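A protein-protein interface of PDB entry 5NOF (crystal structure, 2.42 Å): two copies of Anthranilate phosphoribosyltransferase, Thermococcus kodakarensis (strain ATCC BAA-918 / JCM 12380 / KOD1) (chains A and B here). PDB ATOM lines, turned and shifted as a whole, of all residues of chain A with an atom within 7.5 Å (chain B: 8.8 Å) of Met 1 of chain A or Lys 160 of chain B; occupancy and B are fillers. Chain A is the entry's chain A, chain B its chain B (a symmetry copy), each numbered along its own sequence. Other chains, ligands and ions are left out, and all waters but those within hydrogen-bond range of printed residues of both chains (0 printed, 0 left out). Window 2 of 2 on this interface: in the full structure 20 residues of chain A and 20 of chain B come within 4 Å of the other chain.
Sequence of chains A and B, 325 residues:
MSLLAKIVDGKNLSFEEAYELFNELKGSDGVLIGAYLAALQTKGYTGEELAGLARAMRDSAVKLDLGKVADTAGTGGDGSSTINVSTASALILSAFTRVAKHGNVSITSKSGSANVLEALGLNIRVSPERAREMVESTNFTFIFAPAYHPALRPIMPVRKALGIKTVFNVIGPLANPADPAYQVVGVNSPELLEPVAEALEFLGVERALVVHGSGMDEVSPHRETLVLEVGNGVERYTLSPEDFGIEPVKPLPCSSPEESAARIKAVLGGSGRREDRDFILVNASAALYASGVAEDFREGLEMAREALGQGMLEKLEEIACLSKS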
ATOM      1  N   MET A   1      13.226 -23.740  -7.941  1.00  0.00           N
ATOM      2  CA  MET A   1      13.114 -22.356  -8.462  1.00  0.00           C
ATOM      3  C   MET A   1      11.727 -21.984  -9.049  1.00  0.00           C
ATOM      4  O   MET A   1      11.545 -20.891  -9.584  1.00  0.00           O
ATOM      5  CB  MET A   1      14.216 -22.124  -9.504  1.00  0.00           C
ATOM      6  CG  MET A   1      15.628 -22.271  -8.929  1.00  0.00           C
ATOM      7  SD  MET A   1      16.405 -23.896  -9.028  1.00  0.00           S
ATOM      8  CE  MET A   1      17.100 -23.859 -10.682  1.00  0.00           C
ATOM      9  N   SER A   2      10.759 -22.896  -8.951  1.00  0.00           N
ATOM     10  CA  SER A   2       9.405 -22.657  -9.424  1.00  0.00           C
ATOM     11  C   SER A   2       8.654 -21.642  -8.537  1.00  0.00           C
ATOM     12  O   SER A   2       7.852 -20.870  -9.065  1.00  0.00           O
ATOM     13  CB  SER A   2       8.645 -23.987  -9.536  1.00  0.00           C
ATOM     14  OG  SER A   2       7.345 -23.832 -10.105  1.00  0.00           O
ATOM     15  N   LEU A   3       8.904 -21.622  -7.218  1.00  0.00           N
ATOM     16  CA  LEU A   3       8.269 -20.603  -6.347  1.00  0.00           C
ATOM     17  C   LEU A   3       8.789 -19.195  -6.678  1.00  0.00           C
ATOM     18  O   LEU A   3       8.003 -18.243  -6.773  1.00  0.00           O
ATOM     19  CB  LEU A   3       8.424 -20.922  -4.849  1.00  0.00           C
ATOM     20  CG  LEU A   3       7.508 -22.039  -4.292  1.00  0.00           C
ATOM     21  CD1 LEU A   3       7.633 -22.197  -2.782  1.00  0.00           C
ATOM     22  CD2 LEU A   3       6.038 -21.828  -4.656  1.00  0.00           C
ATOM     23  N   LEU A   4      10.094 -19.077  -6.910  1.00  0.00           N
ATOM     24  CA  LEU A   4      10.679 -17.815  -7.355  1.00  0.00           C
ATOM     25  C   LEU A   4      10.081 -17.379  -8.684  1.00  0.00           C
ATOM     26  O   LEU A   4       9.678 -16.216  -8.842  1.00  0.00           O
ATOM     27  CB  LEU A   4      12.201 -17.916  -7.478  1.00  0.00           C
ATOM     28  CG  LEU A   4      12.968 -16.638  -7.788  1.00  0.00           C
ATOM     29  CD1 LEU A   4      12.684 -15.600  -6.722  1.00  0.00           C
ATOM     30  CD2 LEU A   4      14.464 -16.948  -7.909  1.00  0.00           C
ATOM     31  N   ALA A   5       9.991 -18.317  -9.622  1.00  0.00           N
ATOM     32  CA  ALA A   5       9.382 -18.030 -10.919  1.00  0.00           C
ATOM     33  C   ALA A   5       7.935 -17.595 -10.767  1.00  0.00           C
ATOM     34  O   ALA A   5       7.477 -16.718 -11.495  1.00  0.00           O
ATOM     35  CB  ALA A   5       9.474 -19.229 -11.837  1.00  0.00           C
ATOM     36  N   LYS A   6       7.221 -18.197  -9.822  1.00  0.00           N
ATOM     37  CA  LYS A   6       5.828 -17.841  -9.579  1.00  0.00           C
ATOM     38  C   LYS A   6       5.726 -16.383  -9.091  1.00  0.00           C
ATOM     39  O   LYS A   6       4.939 -15.581  -9.640  1.00  0.00           O
ATOM     40  CB  LYS A   6       5.185 -18.840  -8.608  1.00  0.00           C
ATOM     41  CG  LYS A   6       3.686 -18.967  -8.703  1.00  0.00           C
ATOM     42  CD  LYS A   6       3.205 -20.278  -8.068  1.00  0.00           C
ATOM     43  CE  LYS A   6       1.679 -20.396  -8.025  1.00  0.00           C
ATOM     44  NZ  LYS A   6       0.975 -19.338  -7.240  1.00  0.00           N
ATOM     45  N   ILE A   7       6.580 -16.029  -8.127  1.00  0.00           N
ATOM     46  CA  ILE A   7       6.648 -14.658  -7.550  1.00  0.00           C
ATOM     47  C   ILE A   7       7.026 -13.574  -8.581  1.00  0.00           C
ATOM     48  O   ILE A   7       6.414 -12.516  -8.640  1.00  0.00           O
ATOM     49  CB  ILE A   7       7.658 -14.602  -6.368  1.00  0.00           C
ATOM     50  CG1 ILE A   7       7.174 -15.426  -5.184  1.00  0.00           C
ATOM     51  CG2 ILE A   7       7.943 -13.165  -5.923  1.00  0.00           C
ATOM     52  CD1 ILE A   7       8.308 -15.874  -4.282  1.00  0.00           C
ATOM     53  N   GLU A  24      12.117 -23.958   2.465  1.00  0.00           N
ATOM     54  CA  GLU A  24      13.126 -23.770   1.424  1.00  0.00           C
ATOM     55  C   GLU A  24      14.138 -22.658   1.767  1.00  0.00           C
ATOM     56  O   GLU A  24      15.332 -22.831   1.545  1.00  0.00           O
ATOM     57  CB  GLU A  24      12.472 -23.481   0.064  1.00  0.00           C
ATOM     58  CG  GLU A  24      13.437 -23.655  -1.114  1.00  0.00           C
ATOM     59  CD  GLU A  24      12.874 -23.194  -2.441  1.00  0.00           C
ATOM     60  OE1 GLU A  24      11.705 -23.537  -2.746  1.00  0.00           O
ATOM     61  OE2 GLU A  24      13.619 -22.524  -3.195  1.00  0.00           O
ATOM     62  N   LEU A  32      19.967 -17.256  -3.165  1.00  0.00           N
ATOM     63  CA  LEU A  32      18.568 -17.563  -3.425  1.00  0.00           C
ATOM     64  C   LEU A  32      17.652 -16.869  -2.412  1.00  0.00           C
ATOM     65  O   LEU A  32      16.545 -16.418  -2.756  1.00  0.00           O
ATOM     66  CB  LEU A  32      18.352 -19.069  -3.384  1.00  0.00           C
ATOM     67  CG  LEU A  32      17.171 -19.604  -4.166  1.00  0.00           C
ATOM     68  CD1 LEU A  32      17.427 -19.506  -5.665  1.00  0.00           C
ATOM     69  CD2 LEU A  32      16.898 -21.042  -3.739  1.00  0.00           C
ATOM     70  N   TYR A  36      14.700 -14.242  -3.255  1.00  0.00           N
ATOM     71  CA  TYR A  36      13.344 -14.413  -2.731  1.00  0.00           C
ATOM     72  C   TYR A  36      12.860 -13.176  -1.991  1.00  0.00           C
ATOM     73  O   TYR A  36      11.746 -12.710  -2.226  1.00  0.00           O
ATOM     74  CB  TYR A  36      13.218 -15.671  -1.841  1.00  0.00           C
ATOM     75  CG  TYR A  36      12.893 -16.945  -2.612  1.00  0.00           C
ATOM     76  CD1 TYR A  36      11.680 -17.081  -3.278  1.00  0.00           C
ATOM     77  CD2 TYR A  36      13.795 -18.020  -2.663  1.00  0.00           C
ATOM     78  CE1 TYR A  36      11.366 -18.238  -3.973  1.00  0.00           C
ATOM     79  CE2 TYR A  36      13.493 -19.184  -3.357  1.00  0.00           C
ATOM     80  CZ  TYR A  36      12.279 -19.291  -4.009  1.00  0.00           C
ATOM     81  OH  TYR A  36      11.976 -20.435  -4.712  1.00  0.00           O
ATOM     82  N   LEU B  37      18.692  -9.068  -9.561  1.00  0.00           N
ATOM     83  CA  LEU B  37      18.170  -9.732 -10.748  1.00  0.00           C
ATOM     84  C   LEU B  37      16.718 -10.122 -10.569  1.00  0.00           C
ATOM     85  O   LEU B  37      15.888  -9.854 -11.457  1.00  0.00           O
ATOM     86  CB  LEU B  37      19.021 -10.939 -11.139  1.00  0.00           C
ATOM     87  CG  LEU B  37      20.467 -10.623 -11.572  1.00  0.00           C
ATOM     88  CD1 LEU B  37      21.141 -11.841 -12.189  1.00  0.00           C
ATOM     89  CD2 LEU B  37      20.503  -9.473 -12.561  1.00  0.00           C
ATOM     90  N   VAL B 105      24.143 -15.479 -24.739  1.00  0.00           N
ATOM     91  CA  VAL B 105      24.229 -15.048 -23.350  1.00  0.00           C
ATOM     92  C   VAL B 105      23.661 -16.085 -22.364  1.00  0.00           C
ATOM     93  O   VAL B 105      24.180 -16.241 -21.259  1.00  0.00           O
ATOM     94  CB  VAL B 105      23.483 -13.684 -23.178  1.00  0.00           C
ATOM     95  CG1 VAL B 105      21.971 -13.849 -23.389  1.00  0.00           C
ATOM     96  CG2 VAL B 105      23.780 -13.030 -21.838  1.00  0.00           C
ATOM     97  N   SER B 106      22.646 -16.839 -22.812  1.00  0.00           N
ATOM     98  CA  SER B 106      21.969 -17.872 -21.984  1.00  0.00           C
ATOM     99  C   SER B 106      22.738 -19.208 -21.959  1.00  0.00           C
ATOM    100  O   SER B 106      23.402 -19.568 -22.941  1.00  0.00           O
ATOM    101  CB  SER B 106      20.539 -18.102 -22.492  1.00  0.00           C
ATOM    102  OG  SER B 106      19.782 -18.891 -21.593  1.00  0.00           O
ATOM    103  N   ILE B 107      22.613 -19.944 -20.849  1.00  0.00           N
ATOM    104  CA  ILE B 107      23.244 -21.274 -20.708  1.00  0.00           C
ATOM    105  C   ILE B 107      22.448 -22.363 -21.441  1.00  0.00           C
ATOM    106  O   ILE B 107      23.027 -23.349 -21.876  1.00  0.00           O
ATOM    107  CB  ILE B 107      23.471 -21.679 -19.218  1.00  0.00           C
ATOM    108  CG1 ILE B 107      24.547 -22.778 -19.078  1.00  0.00           C
ATOM    109  CG2 ILE B 107      22.175 -22.150 -18.564  1.00  0.00           C
ATOM    110  CD1 ILE B 107      25.980 -22.312 -19.254  1.00  0.00           C
ATOM    111  N   THR B 108      21.130 -22.188 -21.531  1.00  0.00           N
ATOM    112  CA  THR B 108      20.239 -23.178 -22.156  1.00  0.00           C
ATOM    113  C   THR B 108      20.446 -23.188 -23.679  1.00  0.00           C
ATOM    114  O   THR B 108      19.632 -22.627 -24.438  1.00  0.00           O
ATOM    115  CB  THR B 108      18.748 -22.910 -21.810  1.00  0.00           C
ATOM    116  OG1 THR B 108      18.579 -22.910 -20.387  1.00  0.00           O
ATOM    117  CG2 THR B 108      17.823 -23.982 -22.418  1.00  0.00           C
ATOM    118  N   SER B 109      21.545 -23.805 -24.123  1.00  0.00           N
ATOM    119  CA  SER B 109      21.926 -23.800 -25.544  1.00  0.00           C
ATOM    120  C   SER B 109      21.733 -25.044 -26.430  1.00  0.00           C
ATOM    121  O   SER B 109      22.586 -25.351 -27.263  1.00  0.00           O
ATOM    122  CB  SER B 109      23.375 -23.309 -25.684  1.00  0.00           C
ATOM    123  OG  SER B 109      23.420 -22.010 -26.248  1.00  0.00           O
ATOM    124  N   LEU B 152      30.936 -10.732 -16.550  1.00  0.00           N
ATOM    125  CA  LEU B 152      29.863 -11.697 -16.271  1.00  0.00           C
ATOM    126  C   LEU B 152      30.270 -12.933 -15.473  1.00  0.00           C
ATOM    127  O   LEU B 152      29.408 -13.641 -14.978  1.00  0.00           O
ATOM    128  CB  LEU B 152      29.254 -12.189 -17.578  1.00  0.00           C
ATOM    129  CG  LEU B 152      28.551 -11.167 -18.478  1.00  0.00           C
ATOM    130  CD1 LEU B 152      27.868 -11.916 -19.621  1.00  0.00           C
ATOM    131  CD2 LEU B 152      27.557 -10.312 -17.713  1.00  0.00           C
ATOM    132  N   PRO B 154      31.363 -13.577 -12.388  1.00  0.00           N
ATOM    133  CA  PRO B 154      30.594 -13.682 -11.129  1.00  0.00           C
ATOM    134  C   PRO B 154      29.069 -13.719 -11.272  1.00  0.00           C
ATOM    135  O   PRO B 154      28.394 -14.281 -10.409  1.00  0.00           O
ATOM    136  CB  PRO B 154      30.984 -12.406 -10.354  1.00  0.00           C
ATOM    137  CG  PRO B 154      32.226 -11.905 -10.988  1.00  0.00           C
ATOM    138  CD  PRO B 154      32.136 -12.323 -12.428  1.00  0.00           C
ATOM    139  N   ILE B 155      28.522 -13.090 -12.317  1.00  0.00           N
ATOM    140  CA  ILE B 155      27.068 -13.100 -12.573  1.00  0.00           C
ATOM    141  C   ILE B 155      26.525 -14.490 -12.984  1.00  0.00           C
ATOM    142  O   ILE B 155      25.394 -14.800 -12.652  1.00  0.00           O
ATOM    143  CB  ILE B 155      26.689 -11.966 -13.582  1.00  0.00           C
ATOM    144  CG1 ILE B 155      26.704 -10.608 -12.847  1.00  0.00           C
ATOM    145  CG2 ILE B 155      25.303 -12.137 -14.204  1.00  0.00           C
ATOM    146  CD1 ILE B 155      27.978  -9.793 -12.943  1.00  0.00           C
ATOM    147  N   MET B 156      27.311 -15.311 -13.692  1.00  0.00           N
ATOM    148  CA  MET B 156      26.805 -16.576 -14.245  1.00  0.00           C
ATOM    149  C   MET B 156      26.348 -17.624 -13.221  1.00  0.00           C
ATOM    150  O   MET B 156      25.296 -18.222 -13.410  1.00  0.00           O
ATOM    151  CB  MET B 156      27.796 -17.199 -15.251  1.00  0.00           C
ATOM    152  CG  MET B 156      27.929 -16.437 -16.572  1.00  0.00           C
ATOM    153  SD  MET B 156      26.401 -16.133 -17.509  1.00  0.00           S
ATOM    154  CE  MET B 156      27.023 -15.034 -18.787  1.00  0.00           C
ATOM    155  N   PRO B 157      27.127 -17.851 -12.146  1.00  0.00           N
ATOM    156  CA  PRO B 157      26.660 -18.760 -11.074  1.00  0.00           C
ATOM    157  C   PRO B 157      25.315 -18.343 -10.482  1.00  0.00           C
ATOM    158  O   PRO B 157      24.452 -19.200 -10.223  1.00  0.00           O
ATOM    159  CB  PRO B 157      27.749 -18.651  -9.999  1.00  0.00           C
ATOM    160  CG  PRO B 157      28.954 -18.139 -10.712  1.00  0.00           C
ATOM    161  CD  PRO B 157      28.467 -17.315 -11.863  1.00  0.00           C
ATOM    162  N   VAL B 158      25.145 -17.037 -10.303  1.00  0.00           N
ATOM    163  CA  VAL B 158      23.926 -16.489  -9.726  1.00  0.00           C
ATOM    164  C   VAL B 158      22.742 -16.728 -10.664  1.00  0.00           C
ATOM    165  O   VAL B 158      21.651 -17.035 -10.204  1.00  0.00           O
ATOM    166  CB  VAL B 158      24.071 -14.984  -9.390  1.00  0.00           C
ATOM    167  CG1 VAL B 158      22.756 -14.424  -8.849  1.00  0.00           C
ATOM    168  CG2 VAL B 158      25.236 -14.770  -8.425  1.00  0.00           C
ATOM    169  N   ARG B 159      22.962 -16.622 -11.969  1.00  0.00           N
ATOM    170  CA  ARG B 159      21.907 -16.915 -12.941  1.00  0.00           C
ATOM    171  C   ARG B 159      21.515 -18.382 -12.982  1.00  0.00           C
ATOM    172  O   ARG B 159      20.366 -18.681 -13.278  1.00  0.00           O
ATOM    173  CB  ARG B 159      22.312 -16.476 -14.351  1.00  0.00           C
ATOM    174  CG  ARG B 159      22.420 -14.966 -14.505  1.00  0.00           C
ATOM    175  CD  ARG B 159      22.998 -14.624 -15.864  1.00  0.00           C
ATOM    176  NE  ARG B 159      22.100 -15.016 -16.943  1.00  0.00           N
ATOM    177  CZ  ARG B 159      22.415 -15.004 -18.237  1.00  0.00           C
ATOM    178  NH1 ARG B 159      23.632 -14.627 -18.630  1.00  0.00           N
ATOM    179  NH2 ARG B 159      21.515 -15.378 -19.158  1.00  0.00           N
ATOM    180  N   LYS B 160      22.466 -19.290 -12.731  1.00  0.00           N
ATOM    181  CA  LYS B 160      22.165 -20.737 -12.698  1.00  0.00           C
ATOM    182  C   LYS B 160      21.390 -21.076 -11.431  1.00  0.00           C
ATOM    183  O   LYS B 160      20.361 -21.729 -11.498  1.00  0.00           O
ATOM    184  CB  LYS B 160      23.427 -21.625 -12.790  1.00  0.00           C
ATOM    185  CG  LYS B 160      24.324 -21.454 -14.028  1.00  0.00           C
ATOM    186  CD  LYS B 160      23.594 -21.325 -15.372  1.00  0.00           C
ATOM    187  CE  LYS B 160      23.550 -19.884 -15.908  1.00  0.00           C
ATOM    188  NZ  LYS B 160      22.356 -19.505 -16.732  1.00  0.00           N
ATOM    189  N   ALA B 161      21.879 -20.618 -10.286  1.00  0.00           N
ATOM    190  CA  ALA B 161      21.203 -20.849  -9.000  1.00  0.00           C
ATOM    191  C   ALA B 161      19.747 -20.369  -8.975  1.00  0.00           C
ATOM    192  O   ALA B 161      18.897 -21.042  -8.410  1.00  0.00           O
ATOM    193  CB  ALA B 161      21.983 -20.197  -7.866  1.00  0.00           C
ATOM    194  N   LEU B 162      19.472 -19.214  -9.590  1.00  0.00           N
ATOM    195  CA  LEU B 162      18.129 -18.621  -9.607  1.00  0.00           C
ATOM    196  C   LEU B 162      17.166 -19.378 -10.517  1.00  0.00           C
ATOM    197  O   LEU B 162      15.999 -19.551 -10.181  1.00  0.00           O
ATOM    198  CB  LEU B 162      18.187 -17.152 -10.043  1.00  0.00           C
ATOM    199  CG  LEU B 162      18.539 -16.081  -8.997  1.00  0.00           C
ATOM    200  CD1 LEU B 162      19.412 -16.565  -7.852  1.00  0.00           C
ATOM    201  CD2 LEU B 162      19.157 -14.872  -9.676  1.00  0.00           C
ATOM    202  N   GLY B 163      17.659 -19.797 -11.674  1.00  0.00           N
ATOM    203  CA  GLY B 163      16.856 -20.538 -12.647  1.00  0.00           C
ATOM    204  C   GLY B 163      15.573 -19.826 -13.036  1.00  0.00           C
ATOM    205  O   GLY B 163      14.489 -20.424 -13.008  1.00  0.00           O
ATOM    206  N   ILE B 164      15.700 -18.534 -13.335  1.00  0.00           N
ATOM    207  CA  ILE B 164      14.624 -17.756 -13.934  1.00  0.00           C
ATOM    208  C   ILE B 164      15.202 -16.947 -15.084  1.00  0.00           C
ATOM    209  O   ILE B 164      16.412 -16.785 -15.187  1.00  0.00           O
ATOM    210  CB  ILE B 164      13.917 -16.817 -12.916  1.00  0.00           C
ATOM    211  CG1 ILE B 164      14.932 -16.011 -12.107  1.00  0.00           C
ATOM    212  CG2 ILE B 164      13.009 -17.608 -11.986  1.00  0.00           C
ATOM    213  CD1 ILE B 164      14.367 -14.768 -11.461  1.00  0.00           C
ATOM    214  N   LYS B 165      14.320 -16.436 -15.934  1.00  0.00           N
ATOM    215  CA  LYS B 165      14.685 -15.407 -16.907  1.00  0.00           C
ATOM    216  C   LYS B 165      15.120 -14.175 -16.108  1.00  0.00           C
ATOM    217  O   LYS B 165      14.478 -13.817 -15.113  1.00  0.00           O
ATOM    218  CB  LYS B 165      13.504 -15.060 -17.818  1.00  0.00           C
ATOM    219  CG  LYS B 165      13.159 -16.232 -18.723  1.00  0.00           C
ATOM    220  CD  LYS B 165      12.073 -15.869 -19.708  1.00  0.00           C
ATOM    221  CE  LYS B 165      11.847 -16.965 -20.749  1.00  0.00           C
ATOM    222  NZ  LYS B 165      10.911 -18.051 -20.330  1.00  0.00           N
ATOM    223  N   THR B 166      16.233 -13.572 -16.509  1.00  0.00           N
ATOM    224  CA  THR B 166      16.675 -12.305 -15.917  1.00  0.00           C
ATOM    225  C   THR B 166      16.827 -11.296 -17.036  1.00  0.00           C
ATOM    226  O   THR B 166      16.618 -11.611 -18.198  1.00  0.00           O
ATOM    227  CB  THR B 166      18.028 -12.422 -15.179  1.00  0.00           C
ATOM    228  OG1 THR B 166      19.081 -12.519 -16.133  1.00  0.00           O
ATOM    229  CG2 THR B 166      18.054 -13.618 -14.263  1.00  0.00           C
ATOM    230  N   PHE B 168      19.574 -10.321 -18.159  1.00  0.00           N
ATOM    231  CA  PHE B 168      20.698 -10.720 -18.989  1.00  0.00           C
ATOM    232  C   PHE B 168      20.306 -11.474 -20.253  1.00  0.00           C
ATOM    233  O   PHE B 168      21.051 -11.451 -21.236  1.00  0.00           O
ATOM    234  CB  PHE B 168      21.753 -11.473 -18.166  1.00  0.00           C
ATOM    235  CG  PHE B 168      22.596 -10.546 -17.351  1.00  0.00           C
ATOM    236  CD1 PHE B 168      23.638  -9.829 -17.948  1.00  0.00           C
ATOM    237  CD2 PHE B 168      22.312 -10.315 -16.010  1.00  0.00           C
ATOM    238  CE1 PHE B 168      24.385  -8.932 -17.225  1.00  0.00           C
ATOM    239  CE2 PHE B 168      23.084  -9.430 -15.271  1.00  0.00           C
ATOM    240  CZ  PHE B 168      24.132  -8.747 -15.873  1.00  0.00           C
ATOM    241  N   ASN B 169      19.138 -12.118 -20.229  1.00  0.00           N
ATOM    242  CA  ASN B 169      18.534 -12.653 -21.451  1.00  0.00           C
ATOM    243  C   ASN B 169      18.255 -11.570 -22.498  1.00  0.00           C
ATOM    244  O   ASN B 169      18.436 -11.788 -23.695  1.00  0.00           O
ATOM    245  CB  ASN B 169      17.235 -13.404 -21.144  1.00  0.00           C
ATOM    246  CG  ASN B 169      17.482 -14.802 -20.598  1.00  0.00           C
ATOM    247  OD1 ASN B 169      17.690 -14.989 -19.400  1.00  0.00           O
ATOM    248  ND2 ASN B 169      17.463 -15.795 -21.487  1.00  0.00           N
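The backbone NH of Leu 4 of chain A lies within hydrogen-bond range of the side-chain hydroxyl of Tyr 36 of chain A (3.2 Å).
Among the printed residues, merely in contact across the chains: Met 1 of chain A with Leu 162 of chain B, Leu 32 of chain A with Ala 161 of chain B, Met 1 of chain A with Ala 161 of chain B, Leu 4 of chain A with Leu 162 of chain B, Ala 5 of chain A with Ile 164 of chain B, Met 1 of chain A with Gly 163 of chain B and Met 1 of chain A with Lys 160 of chain B.
No position is printed for both chains. Of the 7 pairs that touch across the chains among the printed residues, none has its exchanged pair printed and touching as well.
Met 1 of chain A touches just these residues of chain B: Lys 160, Ala 161, Leu 162 and Gly 163. Of the printed residues of chain A, Leu 162 of chain B touches Met 1 (3.0 Å) and Leu 4 (3.8 Å). Of the printed residues of chain A, Ala 161 of chain B touches Met 1 (3.5 Å) and Leu 32 (3.5 Å). Of the printed residues of chain B, Ala 5 of chain A touches Ile 164 (3.8 Å). Printed residues of chain B within 4 Å of Leu 32 of chain A: Ala 161 (3.5 Å). The nearest residue of chain B that does not touch Met 1 of chain A is Ile 164 of chain B (4.3 Å).
Of the 10 printed residues of chain A, 4 touch a printed residue of chain B. Of the 22 printed residues of chain B, 5 touch a printed residue of chain A. Among the printed residues, 7 pairs touch across the chains. Among the printed residues, no Asp or Glu carboxylate lies within 4 Å of a Lys or Arg side-chain nitrogen of the other chain.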
